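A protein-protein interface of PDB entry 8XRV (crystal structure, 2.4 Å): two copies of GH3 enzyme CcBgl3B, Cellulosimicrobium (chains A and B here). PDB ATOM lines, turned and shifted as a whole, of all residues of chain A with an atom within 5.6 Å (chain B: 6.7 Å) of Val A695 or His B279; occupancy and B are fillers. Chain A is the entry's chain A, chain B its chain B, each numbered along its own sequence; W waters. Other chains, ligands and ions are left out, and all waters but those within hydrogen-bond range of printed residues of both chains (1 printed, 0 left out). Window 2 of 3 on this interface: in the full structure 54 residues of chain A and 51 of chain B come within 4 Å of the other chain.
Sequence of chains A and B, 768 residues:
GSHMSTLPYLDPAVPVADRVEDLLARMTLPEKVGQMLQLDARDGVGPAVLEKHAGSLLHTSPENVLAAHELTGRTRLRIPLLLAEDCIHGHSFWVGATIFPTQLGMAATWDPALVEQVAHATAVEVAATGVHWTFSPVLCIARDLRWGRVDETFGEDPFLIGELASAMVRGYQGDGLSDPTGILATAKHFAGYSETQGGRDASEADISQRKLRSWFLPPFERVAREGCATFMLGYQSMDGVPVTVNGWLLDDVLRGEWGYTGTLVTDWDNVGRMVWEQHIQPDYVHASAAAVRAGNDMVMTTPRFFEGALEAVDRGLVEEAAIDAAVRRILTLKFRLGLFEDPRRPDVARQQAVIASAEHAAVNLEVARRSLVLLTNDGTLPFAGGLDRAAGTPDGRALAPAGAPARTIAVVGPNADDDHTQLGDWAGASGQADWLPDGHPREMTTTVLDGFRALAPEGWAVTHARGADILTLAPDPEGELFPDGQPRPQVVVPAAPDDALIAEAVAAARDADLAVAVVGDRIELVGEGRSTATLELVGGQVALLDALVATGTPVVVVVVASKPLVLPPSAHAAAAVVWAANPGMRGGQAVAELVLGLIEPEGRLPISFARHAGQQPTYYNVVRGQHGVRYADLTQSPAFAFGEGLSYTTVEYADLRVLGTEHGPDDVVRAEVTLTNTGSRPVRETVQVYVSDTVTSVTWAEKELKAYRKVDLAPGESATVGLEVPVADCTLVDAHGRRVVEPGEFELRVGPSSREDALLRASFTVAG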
ATOM      1  N   ARG A 624     -14.592  -0.041   8.315  1.00  0.00           N
ATOM      2  CA  ARG A 624     -15.780   0.744   8.015  1.00  0.00           C
ATOM      3  C   ARG A 624     -16.771  -0.057   7.187  1.00  0.00           C
ATOM      4  O   ARG A 624     -16.434  -1.092   6.597  1.00  0.00           O
ATOM      5  CB  ARG A 624     -15.420   1.992   7.219  1.00  0.00           C
ATOM      6  CG  ARG A 624     -14.495   2.961   7.876  1.00  0.00           C
ATOM      7  CD  ARG A 624     -13.758   3.633   6.751  1.00  0.00           C
ATOM      8  NE  ARG A 624     -12.913   4.720   7.212  1.00  0.00           N
ATOM      9  CZ  ARG A 624     -11.718   4.996   6.706  1.00  0.00           C
ATOM     10  NH1 ARG A 624     -11.233   4.256   5.713  1.00  0.00           N
ATOM     11  NH2 ARG A 624     -11.018   6.017   7.193  1.00  0.00           N
ATOM     12  N   ASP A 693      -7.014   6.877   7.259  1.00  0.00           N
ATOM     13  CA  ASP A 693      -6.996   7.058   5.809  1.00  0.00           C
ATOM     14  C   ASP A 693      -8.416   7.402   5.350  1.00  0.00           C
ATOM     15  O   ASP A 693      -9.270   6.523   5.237  1.00  0.00           O
ATOM     16  CB  ASP A 693      -6.468   5.791   5.145  1.00  0.00           C
ATOM     17  CG  ASP A 693      -6.138   5.985   3.678  1.00  0.00           C
ATOM     18  OD1 ASP A 693      -6.651   6.944   3.079  1.00  0.00           O
ATOM     19  OD2 ASP A 693      -5.386   5.167   3.110  1.00  0.00           O
ATOM     20  N   THR A 694      -8.648   8.684   5.035  1.00  0.00           N
ATOM     21  CA  THR A 694     -10.000   9.200   4.818  1.00  0.00           C
ATOM     22  C   THR A 694     -10.740   8.458   3.707  1.00  0.00           C
ATOM     23  O   THR A 694     -11.907   8.087   3.871  1.00  0.00           O
ATOM     24  CB  THR A 694      -9.940  10.692   4.510  1.00  0.00           C
ATOM     25  OG1 THR A 694      -9.197  11.357   5.539  1.00  0.00           O
ATOM     26  CG2 THR A 694     -11.347  11.300   4.432  1.00  0.00           C
ATOM     27  N   VAL A 695     -10.099   8.245   2.560  1.00  0.00           N
ATOM     28  CA  VAL A 695     -10.714   7.502   1.465  1.00  0.00           C
ATOM     29  C   VAL A 695      -9.719   6.458   0.979  1.00  0.00           C
ATOM     30  O   VAL A 695      -8.531   6.750   0.824  1.00  0.00           O
ATOM     31  CB  VAL A 695     -11.155   8.420   0.307  1.00  0.00           C
ATOM     32  CG1 VAL A 695     -11.845   7.604  -0.787  1.00  0.00           C
ATOM     33  CG2 VAL A 695     -12.078   9.513   0.812  1.00  0.00           C
ATOM     34  N   THR A 696     -10.193   5.242   0.752  1.00  0.00           N
ATOM     35  CA  THR A 696      -9.323   4.125   0.433  1.00  0.00           C
ATOM     36  C   THR A 696      -9.876   3.411  -0.790  1.00  0.00           C
ATOM     37  O   THR A 696     -11.043   3.566  -1.134  1.00  0.00           O
ATOM     38  CB  THR A 696      -9.203   3.161   1.642  1.00  0.00           C
ATOM     39  OG1 THR A 696     -10.474   2.566   1.942  1.00  0.00           O
ATOM     40  CG2 THR A 696      -8.712   3.892   2.885  1.00  0.00           C
ATOM     41  N   SER A 697      -9.043   2.638  -1.474  1.00  0.00           N
ATOM     42  CA  SER A 697      -9.582   1.908  -2.620  1.00  0.00           C
ATOM     43  C   SER A 697     -10.327   0.654  -2.191  1.00  0.00           C
ATOM     44  O   SER A 697     -11.141   0.124  -2.955  1.00  0.00           O
ATOM     45  CB  SER A 697      -8.462   1.543  -3.603  1.00  0.00           C
ATOM     46  OG  SER A 697      -7.554   0.605  -3.047  1.00  0.00           O
ATOM     47  N   VAL A 698     -10.055   0.170  -0.984  1.00  0.00           N
ATOM     48  CA  VAL A 698     -10.703  -0.990  -0.404  1.00  0.00           C
ATOM     49  C   VAL A 698     -11.175  -0.560   0.968  1.00  0.00           C
ATOM     50  O   VAL A 698     -10.671   0.411   1.534  1.00  0.00           O
ATOM     51  CB  VAL A 698      -9.744  -2.182  -0.298  1.00  0.00           C
ATOM     52  CG1 VAL A 698      -9.478  -2.753  -1.681  1.00  0.00           C
ATOM     53  CG2 VAL A 698      -8.448  -1.720   0.373  1.00  0.00           C
ATOM     54  N   GLU A 742      -1.409   4.688  -0.134  1.00  0.00           N
ATOM     55  CA  GLU A 742      -2.227   5.236  -1.200  1.00  0.00           C
ATOM     56  C   GLU A 742      -2.256   6.749  -1.077  1.00  0.00           C
ATOM     57  O   GLU A 742      -2.636   7.264  -0.018  1.00  0.00           O
ATOM     58  CB  GLU A 742      -3.629   4.682  -1.134  1.00  0.00           C
ATOM     59  CG  GLU A 742      -3.712   3.248  -1.556  1.00  0.00           C
ATOM     60  CD  GLU A 742      -5.137   2.822  -1.839  1.00  0.00           C
ATOM     61  OE1 GLU A 742      -6.090   3.573  -1.476  1.00  0.00           O
ATOM     62  OE2 GLU A 742      -5.292   1.741  -2.451  1.00  0.00           O
ATOM     63  N   GLU A 745      -5.754  12.053   1.313  1.00  0.00           N
ATOM     64  CA  GLU A 745      -5.939  12.711   2.598  1.00  0.00           C
ATOM     65  C   GLU A 745      -5.910  11.720   3.765  1.00  0.00           C
ATOM     66  O   GLU A 745      -6.318  10.556   3.642  1.00  0.00           O
ATOM     67  CB  GLU A 745      -7.256  13.482   2.568  1.00  0.00           C
ATOM     68  CG  GLU A 745      -8.392  12.609   2.078  1.00  0.00           C
ATOM     69  CD  GLU A 745      -9.685  13.374   1.746  1.00  0.00           C
ATOM     70  OE1 GLU A 745     -10.144  14.177   2.595  1.00  0.00           O
ATOM     71  OE2 GLU A 745     -10.232  13.158   0.631  1.00  0.00           O
ATOM     72  N   ARG B 273     -23.447   4.477  -1.718  1.00  0.00           N
ATOM     73  CA  ARG B 273     -22.826   4.066  -0.436  1.00  0.00           C
ATOM     74  C   ARG B 273     -21.308   3.920  -0.620  1.00  0.00           C
ATOM     75  O   ARG B 273     -20.584   4.082   0.370  1.00  0.00           O
ATOM     76  CB  ARG B 273     -23.466   2.767   0.075  1.00  0.00           C
ATOM     77  CG  ARG B 273     -24.831   2.919   0.727  1.00  0.00           C
ATOM     78  CD  ARG B 273     -25.666   1.694   0.408  1.00  0.00           C
ATOM     79  NE  ARG B 273     -26.739   1.298   1.306  1.00  0.00           N
ATOM     80  CZ  ARG B 273     -27.953   1.834   1.379  1.00  0.00           C
ATOM     81  NH1 ARG B 273     -28.835   1.359   2.239  1.00  0.00           N
ATOM     82  NH2 ARG B 273     -28.269   2.880   0.650  1.00  0.00           N
ATOM     83  N   MET B 274     -20.848   3.629  -1.836  1.00  0.00           N
ATOM     84  CA  MET B 274     -19.412   3.536  -2.069  1.00  0.00           C
ATOM     85  C   MET B 274     -18.718   4.854  -1.747  1.00  0.00           C
ATOM     86  O   MET B 274     -17.540   4.867  -1.365  1.00  0.00           O
ATOM     87  CB  MET B 274     -19.176   3.136  -3.521  1.00  0.00           C
ATOM     88  CG  MET B 274     -19.621   1.720  -3.815  1.00  0.00           C
ATOM     89  SD  MET B 274     -18.718   0.972  -5.164  1.00  0.00           S
ATOM     90  CE  MET B 274     -19.355   1.878  -6.564  1.00  0.00           C
ATOM     91  N   VAL B 275     -19.440   5.966  -1.872  1.00  0.00           N
ATOM     92  CA  VAL B 275     -18.913   7.268  -1.496  1.00  0.00           C
ATOM     93  C   VAL B 275     -19.024   7.453   0.014  1.00  0.00           C
ATOM     94  O   VAL B 275     -18.010   7.468   0.721  1.00  0.00           O
ATOM     95  CB  VAL B 275     -19.632   8.402  -2.249  1.00  0.00           C
ATOM     96  CG1 VAL B 275     -18.922   9.714  -2.000  1.00  0.00           C
ATOM     97  CG2 VAL B 275     -19.695   8.091  -3.730  1.00  0.00           C
ATOM     98  N   TRP B 276     -20.253   7.577   0.527  1.00  0.00           N
ATOM     99  CA  TRP B 276     -20.438   8.113   1.875  1.00  0.00           C
ATOM    100  C   TRP B 276     -20.430   7.068   2.992  1.00  0.00           C
ATOM    101  O   TRP B 276     -20.484   7.449   4.167  1.00  0.00           O
ATOM    102  CB  TRP B 276     -21.735   8.923   1.950  1.00  0.00           C
ATOM    103  CG  TRP B 276     -22.985   8.160   1.610  1.00  0.00           C
ATOM    104  CD1 TRP B 276     -23.612   8.101   0.392  1.00  0.00           C
ATOM    105  CD2 TRP B 276     -23.787   7.381   2.509  1.00  0.00           C
ATOM    106  NE1 TRP B 276     -24.746   7.321   0.476  1.00  0.00           N
ATOM    107  CE2 TRP B 276     -24.873   6.865   1.764  1.00  0.00           C
ATOM    108  CE3 TRP B 276     -23.690   7.064   3.871  1.00  0.00           C
ATOM    109  CZ2 TRP B 276     -25.854   6.039   2.339  1.00  0.00           C
ATOM    110  CZ3 TRP B 276     -24.663   6.243   4.441  1.00  0.00           C
ATOM    111  CH2 TRP B 276     -25.730   5.739   3.672  1.00  0.00           C
ATOM    112  N   GLU B 277     -20.347   5.797   2.691  1.00  0.00           N
ATOM    113  CA  GLU B 277     -20.435   4.865   3.814  1.00  0.00           C
ATOM    114  C   GLU B 277     -19.275   3.877   3.863  1.00  0.00           C
ATOM    115  O   GLU B 277     -18.776   3.549   4.949  1.00  0.00           O
ATOM    116  CB  GLU B 277     -21.773   4.112   3.742  1.00  0.00           C
ATOM    117  CG  GLU B 277     -22.258   3.577   5.073  1.00  0.00           C
ATOM    118  CD  GLU B 277     -23.693   3.090   4.995  1.00  0.00           C
ATOM    119  OE1 GLU B 277     -24.112   2.678   3.886  1.00  0.00           O
ATOM    120  OE2 GLU B 277     -24.400   3.120   6.035  1.00  0.00           O
ATOM    121  N   GLN B 278     -18.856   3.374   2.715  1.00  0.00           N
ATOM    122  CA  GLN B 278     -17.672   2.545   2.590  1.00  0.00           C
ATOM    123  C   GLN B 278     -16.400   3.354   2.363  1.00  0.00           C
ATOM    124  O   GLN B 278     -15.315   2.888   2.733  1.00  0.00           O
ATOM    125  CB  GLN B 278     -17.952   1.560   1.464  1.00  0.00           C
ATOM    126  CG  GLN B 278     -18.903   0.469   1.900  1.00  0.00           C
ATOM    127  CD  GLN B 278     -19.527  -0.262   0.734  1.00  0.00           C
ATOM    128  OE1 GLN B 278     -19.502   0.225  -0.398  1.00  0.00           O
ATOM    129  NE2 GLN B 278     -19.980  -1.492   0.979  1.00  0.00           N
ATOM    130  N   HIS B 279     -16.523   4.562   1.797  1.00  0.00           N
ATOM    131  CA  HIS B 279     -15.392   5.464   1.566  1.00  0.00           C
ATOM    132  C   HIS B 279     -14.368   4.847   0.618  1.00  0.00           C
ATOM    133  O   HIS B 279     -13.159   4.970   0.821  1.00  0.00           O
ATOM    134  CB  HIS B 279     -14.728   5.882   2.884  1.00  0.00           C
ATOM    135  CG  HIS B 279     -15.625   6.677   3.778  1.00  0.00           C
ATOM    136  ND1 HIS B 279     -16.400   6.098   4.760  1.00  0.00           N
ATOM    137  CD2 HIS B 279     -15.896   8.004   3.818  1.00  0.00           C
ATOM    138  CE1 HIS B 279     -17.102   7.034   5.374  1.00  0.00           C
ATOM    139  NE2 HIS B 279     -16.810   8.200   4.825  1.00  0.00           N
ATOM    140  N   ILE B 280     -14.857   4.168  -0.419  1.00  0.00           N
ATOM    141  CA  ILE B 280     -14.003   3.601  -1.455  1.00  0.00           C
ATOM    142  C   ILE B 280     -14.114   4.344  -2.775  1.00  0.00           C
ATOM    143  O   ILE B 280     -13.470   3.942  -3.754  1.00  0.00           O
ATOM    144  CB  ILE B 280     -14.264   2.095  -1.665  1.00  0.00           C
ATOM    145  CG1 ILE B 280     -15.627   1.857  -2.303  1.00  0.00           C
ATOM    146  CG2 ILE B 280     -14.073   1.311  -0.362  1.00  0.00           C
ATOM    147  CD1 ILE B 280     -15.621   0.654  -3.183  1.00  0.00           C
ATOM    148  N   GLN B 281     -14.910   5.405  -2.839  1.00  0.00           N
ATOM    149  CA  GLN B 281     -14.966   6.293  -3.979  1.00  0.00           C
ATOM    150  C   GLN B 281     -14.946   7.726  -3.469  1.00  0.00           C
ATOM    151  O   GLN B 281     -15.490   8.003  -2.389  1.00  0.00           O
ATOM    152  CB  GLN B 281     -16.224   6.049  -4.823  1.00  0.00           C
ATOM    153  CG  GLN B 281     -16.296   4.651  -5.428  1.00  0.00           C
ATOM    154  CD  GLN B 281     -15.248   4.428  -6.499  1.00  0.00           C
ATOM    155  OE1 GLN B 281     -14.658   5.382  -7.004  1.00  0.00           O
ATOM    156  NE2 GLN B 281     -15.004   3.165  -6.849  1.00  0.00           N
ATOM    157  N   PRO B 282     -14.296   8.657  -4.200  1.00  0.00           N
ATOM    158  CA  PRO B 282     -14.213  10.047  -3.727  1.00  0.00           C
ATOM    159  C   PRO B 282     -15.437  10.877  -4.097  1.00  0.00           C
ATOM    160  O   PRO B 282     -15.763  11.835  -3.390  1.00  0.00           O
ATOM    161  CB  PRO B 282     -12.955  10.571  -4.423  1.00  0.00           C
ATOM    162  CG  PRO B 282     -12.929   9.815  -5.725  1.00  0.00           C
ATOM    163  CD  PRO B 282     -13.562   8.459  -5.467  1.00  0.00           C
HETATM  164  O   HOH W   1     -12.092   1.465  -5.153  1.00  0.00           O
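O of His B279 is in hydrogen-bond range of N of Thr A696, 3.0 Å away.
The backbone carbonyl oxygen (O) of Glu A745 is in hydrogen-bond range of the backbone NH (N) of Thr A694 (3.3 Å).
The side-chain hydroxyl of Ser A697 sits at hydrogen-bond distance from the side-chain carboxylate of Glu A742 (2.6 Å).
The backbone NH (N) of His B279 is in hydrogen-bond range of the backbone carbonyl oxygen (O) of Met B274.
O of Met B274 lies within hydrogen-bond range of N of Ile B280, at 2.9 Å.
The backbone carbonyl oxygen (O) of Glu B277 sits at hydrogen-bond distance from a ring nitrogen (ND1) of His B279 (3.5 Å).
Thr A694 touches His B279.
Val A695 touches His B279 (CG1 to O, 3.4 Å).
O of Thr A696 touches CA of Ile B280 (3.0 Å).
O of Ser A697 touches CB of Ile B280, 3.9 Å away.
C of Val A698 touches CG2 of Ile B280, 3.7 Å away.
Of the printed residues of chain B, Thr A694 touches His B279.
Of the printed residues of chain B, Thr A696 touches His B279 and Ile B280.
Of chain A, only Thr A694 (3.7 Å), Val A695 (3.4 Å) and Thr A696 (3.0 Å) come within 4 Å of His B279.
The nearest printed residue of chain B that does not touch Val A695 is Gln B281 (4.001 Å).
The nearest residue of chain A that does not touch His B279 is Arg A624 (4.1 Å).
Of the 10 printed residues of chain B, 2 touch a printed residue of chain A.
Hydrophobic or aromatic side chains of chain B within 4 Å of the printed part of chain A: His B279 and Ile B280.
Hydrophobic or aromatic side chains of chain A that line the printed part of chain B: Val A695.
Among the printed residues, no Asp or Glu carboxylate lies within 4 Å of a Lys or Arg side-chain nitrogen of the other chain.
No position is printed for both chains.
Of the 6 pairs that touch across the chains among the printed residues, none has its exchanged pair printed and touching as well.
Water W1 lies within hydrogen-bond range of O of Ser A697 (2.7 Å) and O of Ile B280 (3.2 Å).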
